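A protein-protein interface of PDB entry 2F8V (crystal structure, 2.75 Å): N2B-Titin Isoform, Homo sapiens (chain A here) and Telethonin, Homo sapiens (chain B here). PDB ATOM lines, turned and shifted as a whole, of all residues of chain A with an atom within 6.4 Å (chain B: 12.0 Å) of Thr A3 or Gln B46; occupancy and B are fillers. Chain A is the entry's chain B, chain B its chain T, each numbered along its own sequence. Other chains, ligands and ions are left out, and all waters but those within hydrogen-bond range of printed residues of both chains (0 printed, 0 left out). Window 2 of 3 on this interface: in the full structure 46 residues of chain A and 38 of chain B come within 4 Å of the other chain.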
ATOM      1  N   MET A   1      25.286 -21.842  -3.045  1.00  0.00           N
ATOM      2  CA  MET A   1      25.282 -20.355  -3.120  1.00  0.00           C
ATOM      3  C   MET A   1      24.974 -19.766  -1.755  1.00  0.00           C
ATOM      4  O   MET A   1      25.230 -18.584  -1.495  1.00  0.00           O
ATOM      5  CB  MET A   1      24.241 -19.877  -4.135  1.00  0.00           C
ATOM      6  CG  MET A   1      24.580 -20.209  -5.579  1.00  0.00           C
ATOM      7  SD  MET A   1      23.664 -19.196  -6.764  1.00  0.00           S
ATOM      8  CE  MET A   1      24.502 -17.616  -6.614  1.00  0.00           C
ATOM      9  N   THR A   2      24.414 -20.598  -0.890  1.00  0.00           N
ATOM     10  CA  THR A   2      24.051 -20.183   0.450  1.00  0.00           C
ATOM     11  C   THR A   2      24.382 -21.332   1.392  1.00  0.00           C
ATOM     12  O   THR A   2      23.586 -22.262   1.552  1.00  0.00           O
ATOM     13  CB  THR A   2      22.549 -19.863   0.514  1.00  0.00           C
ATOM     14  OG1 THR A   2      21.813 -20.897  -0.156  1.00  0.00           O
ATOM     15  CG2 THR A   2      22.239 -18.589  -0.259  1.00  0.00           C
ATOM     16  N   THR A   3      25.564 -21.279   1.997  1.00  0.00           N
ATOM     17  CA  THR A   3      25.997 -22.345   2.883  1.00  0.00           C
ATOM     18  C   THR A   3      24.956 -22.599   3.968  1.00  0.00           C
ATOM     19  O   THR A   3      24.788 -21.791   4.880  1.00  0.00           O
ATOM     20  CB  THR A   3      27.349 -22.025   3.513  1.00  0.00           C
ATOM     21  OG1 THR A   3      27.756 -23.139   4.312  1.00  0.00           O
ATOM     22  CG2 THR A   3      27.221 -20.863   4.488  1.00  0.00           C
ATOM     23  N   GLN A   4      24.273 -23.739   3.851  1.00  0.00           N
ATOM     24  CA  GLN A   4      23.112 -24.087   4.669  1.00  0.00           C
ATOM     25  C   GLN A   4      23.214 -25.505   5.230  1.00  0.00           C
ATOM     26  O   GLN A   4      23.318 -26.463   4.473  1.00  0.00           O
ATOM     27  CB  GLN A   4      21.849 -23.972   3.805  1.00  0.00           C
ATOM     28  CG  GLN A   4      20.700 -24.879   4.210  1.00  0.00           C
ATOM     29  CD  GLN A   4      19.472 -24.725   3.317  1.00  0.00           C
ATOM     30  OE1 GLN A   4      19.110 -25.651   2.586  1.00  0.00           O
ATOM     31  NE2 GLN A   4      18.827 -23.562   3.377  1.00  0.00           N
ATOM     32  N   ALA A   5      23.161 -25.643   6.553  1.00  0.00           N
ATOM     33  CA  ALA A   5      23.253 -26.954   7.198  1.00  0.00           C
ATOM     34  C   ALA A   5      22.142 -27.892   6.731  1.00  0.00           C
ATOM     35  O   ALA A   5      21.079 -27.437   6.314  1.00  0.00           O
ATOM     36  CB  ALA A   5      23.237 -26.820   8.710  1.00  0.00           C
ATOM     37  N   PHE A  32      23.878 -27.535   1.716  1.00  0.00           N
ATOM     38  CA  PHE A  32      24.889 -27.120   0.770  1.00  0.00           C
ATOM     39  C   PHE A  32      26.153 -26.745   1.542  1.00  0.00           C
ATOM     40  O   PHE A  32      26.092 -25.963   2.483  1.00  0.00           O
ATOM     41  CB  PHE A  32      24.384 -25.938  -0.051  1.00  0.00           C
ATOM     42  CG  PHE A  32      25.233 -25.623  -1.258  1.00  0.00           C
ATOM     43  CD1 PHE A  32      24.782 -25.937  -2.536  1.00  0.00           C
ATOM     44  CD2 PHE A  32      26.473 -25.012  -1.115  1.00  0.00           C
ATOM     45  CE1 PHE A  32      25.556 -25.655  -3.654  1.00  0.00           C
ATOM     46  CE2 PHE A  32      27.256 -24.721  -2.231  1.00  0.00           C
ATOM     47  CZ  PHE A  32      26.797 -25.043  -3.502  1.00  0.00           C
ATOM     48  N   PRO A  33      27.298 -27.320   1.156  1.00  0.00           N
ATOM     49  CA  PRO A  33      27.386 -28.299   0.064  1.00  0.00           C
ATOM     50  C   PRO A  33      26.496 -29.493   0.368  1.00  0.00           C
ATOM     51  O   PRO A  33      26.195 -29.711   1.539  1.00  0.00           O
ATOM     52  CB  PRO A  33      28.854 -28.733   0.105  1.00  0.00           C
ATOM     53  CG  PRO A  33      29.577 -27.629   0.807  1.00  0.00           C
ATOM     54  CD  PRO A  33      28.608 -27.043   1.779  1.00  0.00           C
ATOM     55  N   ASN A  84      27.575 -32.481   6.765  1.00  0.00           N
ATOM     56  CA  ASN A  84      28.184 -31.478   5.917  1.00  0.00           C
ATOM     57  C   ASN A  84      28.930 -30.457   6.783  1.00  0.00           C
ATOM     58  O   ASN A  84      28.860 -30.517   8.009  1.00  0.00           O
ATOM     59  CB  ASN A  84      27.145 -30.880   4.956  1.00  0.00           C
ATOM     60  CG  ASN A  84      26.849 -29.427   5.219  1.00  0.00           C
ATOM     61  OD1 ASN A  84      27.352 -28.837   6.169  1.00  0.00           O
ATOM     62  ND2 ASN A  84      26.026 -28.834   4.362  1.00  0.00           N
ATOM     63  N   GLY A  85      29.669 -29.549   6.162  1.00  0.00           N
ATOM     64  CA  GLY A  85      30.542 -28.657   6.907  1.00  0.00           C
ATOM     65  C   GLY A  85      29.895 -27.708   7.897  1.00  0.00           C
ATOM     66  O   GLY A  85      30.569 -27.190   8.778  1.00  0.00           O
ATOM     67  N   SER A  86      28.598 -27.470   7.775  1.00  0.00           N
ATOM     68  CA  SER A  86      27.925 -26.519   8.655  1.00  0.00           C
ATOM     69  C   SER A  86      27.143 -27.175   9.784  1.00  0.00           C
ATOM     70  O   SER A  86      26.626 -26.497  10.685  1.00  0.00           O
ATOM     71  CB  SER A  86      26.980 -25.653   7.837  1.00  0.00           C
ATOM     72  OG  SER A  86      27.692 -24.934   6.850  1.00  0.00           O
ATOM     73  N   GLY A  87      27.040 -28.494   9.736  1.00  0.00           N
ATOM     74  CA  GLY A  87      26.296 -29.210  10.749  1.00  0.00           C
ATOM     75  C   GLY A  87      25.972 -30.647  10.395  1.00  0.00           C
ATOM     76  O   GLY A  87      26.673 -31.279   9.614  1.00  0.00           O
ATOM     77  N   GLU B  42      18.585 -32.559  14.628  1.00  0.00           N
ATOM     78  CA  GLU B  42      19.418 -31.768  13.730  1.00  0.00           C
ATOM     79  C   GLU B  42      20.311 -30.762  14.483  1.00  0.00           C
ATOM     80  O   GLU B  42      19.860 -30.079  15.423  1.00  0.00           O
ATOM     81  CB  GLU B  42      18.511 -31.019  12.753  1.00  0.00           C
ATOM     82  CG  GLU B  42      17.548 -31.937  12.043  1.00  0.00           C
ATOM     83  CD  GLU B  42      16.815 -31.256  10.908  1.00  0.00           C
ATOM     84  OE1 GLU B  42      16.652 -30.038  10.987  1.00  0.00           O
ATOM     85  OE2 GLU B  42      16.398 -31.933   9.945  1.00  0.00           O
ATOM     86  N   GLU B  43      21.571 -30.680  14.071  1.00  0.00           N
ATOM     87  CA  GLU B  43      22.501 -29.732  14.655  1.00  0.00           C
ATOM     88  C   GLU B  43      23.104 -28.821  13.606  1.00  0.00           C
ATOM     89  O   GLU B  43      23.573 -29.289  12.576  1.00  0.00           O
ATOM     90  CB  GLU B  43      23.598 -30.466  15.400  1.00  0.00           C
ATOM     91  CG  GLU B  43      23.399 -30.409  16.891  1.00  0.00           C
ATOM     92  CD  GLU B  43      23.595 -31.749  17.545  1.00  0.00           C
ATOM     93  OE1 GLU B  43      24.653 -32.385  17.293  1.00  0.00           O
ATOM     94  OE2 GLU B  43      22.689 -32.164  18.305  1.00  0.00           O
ATOM     95  N   ASP B  44      23.057 -27.516  13.868  1.00  0.00           N
ATOM     96  CA  ASP B  44      23.626 -26.523  12.974  1.00  0.00           C
ATOM     97  C   ASP B  44      24.774 -25.833  13.698  1.00  0.00           C
ATOM     98  O   ASP B  44      24.564 -24.914  14.481  1.00  0.00           O
ATOM     99  CB  ASP B  44      22.572 -25.503  12.542  1.00  0.00           C
ATOM    100  CG  ASP B  44      23.084 -24.562  11.459  1.00  0.00           C
ATOM    101  OD1 ASP B  44      24.275 -24.182  11.513  1.00  0.00           O
ATOM    102  OD2 ASP B  44      22.350 -24.181  10.517  1.00  0.00           O
ATOM    103  N   THR B  45      25.992 -26.284  13.422  1.00  0.00           N
ATOM    104  CA  THR B  45      27.161 -25.814  14.157  1.00  0.00           C
ATOM    105  C   THR B  45      27.614 -24.424  13.697  1.00  0.00           C
ATOM    106  O   THR B  45      28.388 -23.750  14.380  1.00  0.00           O
ATOM    107  CB  THR B  45      28.280 -26.800  13.990  1.00  0.00           C
ATOM    108  OG1 THR B  45      28.361 -27.160  12.611  1.00  0.00           O
ATOM    109  CG2 THR B  45      27.940 -28.096  14.691  1.00  0.00           C
ATOM    110  N   GLN B  46      27.122 -24.007  12.536  1.00  0.00           N
ATOM    111  CA  GLN B  46      27.408 -22.690  12.018  1.00  0.00           C
ATOM    112  C   GLN B  46      26.598 -21.629  12.747  1.00  0.00           C
ATOM    113  O   GLN B  46      27.126 -20.595  13.109  1.00  0.00           O
ATOM    114  CB  GLN B  46      27.097 -22.662  10.529  1.00  0.00           C
ATOM    115  CG  GLN B  46      26.792 -21.287   9.970  1.00  0.00           C
ATOM    116  CD  GLN B  46      26.626 -21.313   8.448  1.00  0.00           C
ATOM    117  OE1 GLN B  46      26.644 -20.263   7.802  1.00  0.00           O
ATOM    118  NE2 GLN B  46      26.481 -22.513   7.875  1.00  0.00           N
ATOM    119  N   ARG B  47      25.316 -21.896  12.962  1.00  0.00           N
ATOM    120  CA  ARG B  47      24.418 -20.963  13.624  1.00  0.00           C
ATOM    121  C   ARG B  47      24.115 -21.343  15.073  1.00  0.00           C
ATOM    122  O   ARG B  47      23.287 -20.712  15.715  1.00  0.00           O
ATOM    123  CB  ARG B  47      23.120 -20.855  12.834  1.00  0.00           C
ATOM    124  CG  ARG B  47      23.264 -20.036  11.570  1.00  0.00           C
ATOM    125  CD  ARG B  47      22.193 -20.296  10.529  1.00  0.00           C
ATOM    126  NE  ARG B  47      21.046 -19.381  10.563  1.00  0.00           N
ATOM    127  CZ  ARG B  47      20.923 -18.294  11.333  1.00  0.00           C
ATOM    128  NH1 ARG B  47      21.882 -17.932  12.187  1.00  0.00           N
ATOM    129  NH2 ARG B  47      19.814 -17.559  11.249  1.00  0.00           N
ATOM    130  N   HIS B  48      24.788 -22.365  15.589  1.00  0.00           N
ATOM    131  CA  HIS B  48      24.591 -22.789  16.967  1.00  0.00           C
ATOM    132  C   HIS B  48      23.129 -22.997  17.342  1.00  0.00           C
ATOM    133  O   HIS B  48      22.687 -22.508  18.367  1.00  0.00           O
ATOM    134  CB  HIS B  48      25.215 -21.791  17.923  1.00  0.00           C
ATOM    135  CG  HIS B  48      26.563 -21.317  17.488  1.00  0.00           C
ATOM    136  ND1 HIS B  48      27.480 -22.145  16.871  1.00  0.00           N
ATOM    137  CD2 HIS B  48      27.150 -20.097  17.567  1.00  0.00           C
ATOM    138  CE1 HIS B  48      28.580 -21.463  16.604  1.00  0.00           C
ATOM    139  NE2 HIS B  48      28.402 -20.217  17.004  1.00  0.00           N
ATOM    140  N   GLU B  49      22.394 -23.735  16.516  1.00  0.00           N
ATOM    141  CA  GLU B  49      20.992 -24.070  16.782  1.00  0.00           C
ATOM    142  C   GLU B  49      20.813 -25.572  16.709  1.00  0.00           C
ATOM    143  O   GLU B  49      21.441 -26.229  15.891  1.00  0.00           O
ATOM    144  CB  GLU B  49      20.091 -23.459  15.721  1.00  0.00           C
ATOM    145  CG  GLU B  49      20.490 -22.073  15.270  1.00  0.00           C
ATOM    146  CD  GLU B  49      19.648 -21.623  14.104  1.00  0.00           C
ATOM    147  OE1 GLU B  49      19.534 -20.390  13.870  1.00  0.00           O
ATOM    148  OE2 GLU B  49      19.082 -22.529  13.436  1.00  0.00           O
ATOM    149  N   THR B  50      19.956 -26.118  17.557  1.00  0.00           N
ATOM    150  CA  THR B  50      19.633 -27.527  17.465  1.00  0.00           C
ATOM    151  C   THR B  50      18.126 -27.698  17.505  1.00  0.00           C
ATOM    152  O   THR B  50      17.421 -26.871  18.054  1.00  0.00           O
ATOM    153  CB  THR B  50      20.301 -28.337  18.600  1.00  0.00           C
ATOM    154  OG1 THR B  50      19.690 -28.026  19.858  1.00  0.00           O
ATOM    155  CG2 THR B  50      21.719 -27.911  18.772  1.00  0.00           C
ATOM    156  N   TYR B  51      17.644 -28.774  16.903  1.00  0.00           N
ATOM    157  CA  TYR B  51      16.222 -29.111  16.923  1.00  0.00           C
ATOM    158  C   TYR B  51      16.089 -30.585  17.183  1.00  0.00           C
ATOM    159  O   TYR B  51      16.866 -31.386  16.675  1.00  0.00           O
ATOM    160  CB  TYR B  51      15.555 -28.816  15.583  1.00  0.00           C
ATOM    161  CG  TYR B  51      14.080 -29.117  15.586  1.00  0.00           C
ATOM    162  CD1 TYR B  51      13.207 -28.339  16.326  1.00  0.00           C
ATOM    163  CD2 TYR B  51      13.556 -30.187  14.868  1.00  0.00           C
ATOM    164  CE1 TYR B  51      11.879 -28.603  16.348  1.00  0.00           C
ATOM    165  CE2 TYR B  51      12.201 -30.448  14.873  1.00  0.00           C
ATOM    166  CZ  TYR B  51      11.370 -29.646  15.621  1.00  0.00           C
ATOM    167  OH  TYR B  51      10.001 -29.860  15.669  1.00  0.00           O
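Printed residues of chain A that touch a printed residue of chain B: Thr A3, Ala A5, Ser A86 and Gly A87. Hydrophobic or aromatic side chains of chain A that line the printed part of chain B: Ala A5.
O of Ser A86 lies close to OD1 of Asp B44. The backbone carbonyl oxygen (O) of Ser A86 lies within hydrogen-bond range of the side-chain hydroxyl (OG1) of Thr B45, 2.7 Å away. The side-chain amide nitrogen of Gln B46 sits at hydrogen-bond distance from the side-chain hydroxyl of Ser A86, 2.9 Å away. The backbone NH of Gly A87 sits at hydrogen-bond distance from the side-chain hydroxyl of Thr B45 (3.4 Å).
Among the printed residues, merely in contact across the chains: Gly A87 with Glu B43, Ala A5 with Asp B44 and Thr A3 with Gln B46.
The side-chain hydroxyl (OG1) of Thr A3 sits at hydrogen-bond distance from the side-chain hydroxyl (OG) of Ser A86, at 3.1 Å. The side-chain carboxylate of Asp B44 lies within hydrogen-bond range of the backbone NH of Gln B46, 3.0 Å away. A ring nitrogen (ND1) of His B48 is in hydrogen-bond range of the backbone carbonyl oxygen of Thr B45 (3.1 Å). The side-chain amide oxygen (OD1) of Asn A84 is in hydrogen-bond range of the backbone NH (N) of Ser A86, at 2.4 Å. The side-chain carboxylate (OD1) of Asp B44 is in hydrogen-bond range of the backbone NH (N) of Arg B47 (2.9 Å). N of Asp B44 lies within hydrogen-bond range of O of Glu B49 (2.9 Å).
Thr A3 touches just one residue of chain B: Gln B46. Of chain A, only Thr A3 (3.4 Å) and Ser A86 (2.9 Å) come within 4 Å of Gln B46. No residue of chain B comes within 4 Å of Gln A4. Of chain B, only Asp B44 (3.3 Å) comes within 4 Å of Ala A5. No residue of chain B comes within 4 Å of Pro A33. No residue of chain B comes within 4 Å of Gly A85. Gly A87 touches two residues of chain B. Of the printed residues of chain A, Asp B44 touches Ala A5 (3.3 Å) and Ser A86 (3.4 Å). Of the printed residues of chain A, Thr B45 touches Ser A86 (2.7 Å) and Gly A87 (3.4 Å). Printed residues of chain A within 4 Å of Glu B43: Gly A87 (3.3 Å). The nearest printed residue of chain A that does not touch Gln B46 is Ala A5 (4.8 Å).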
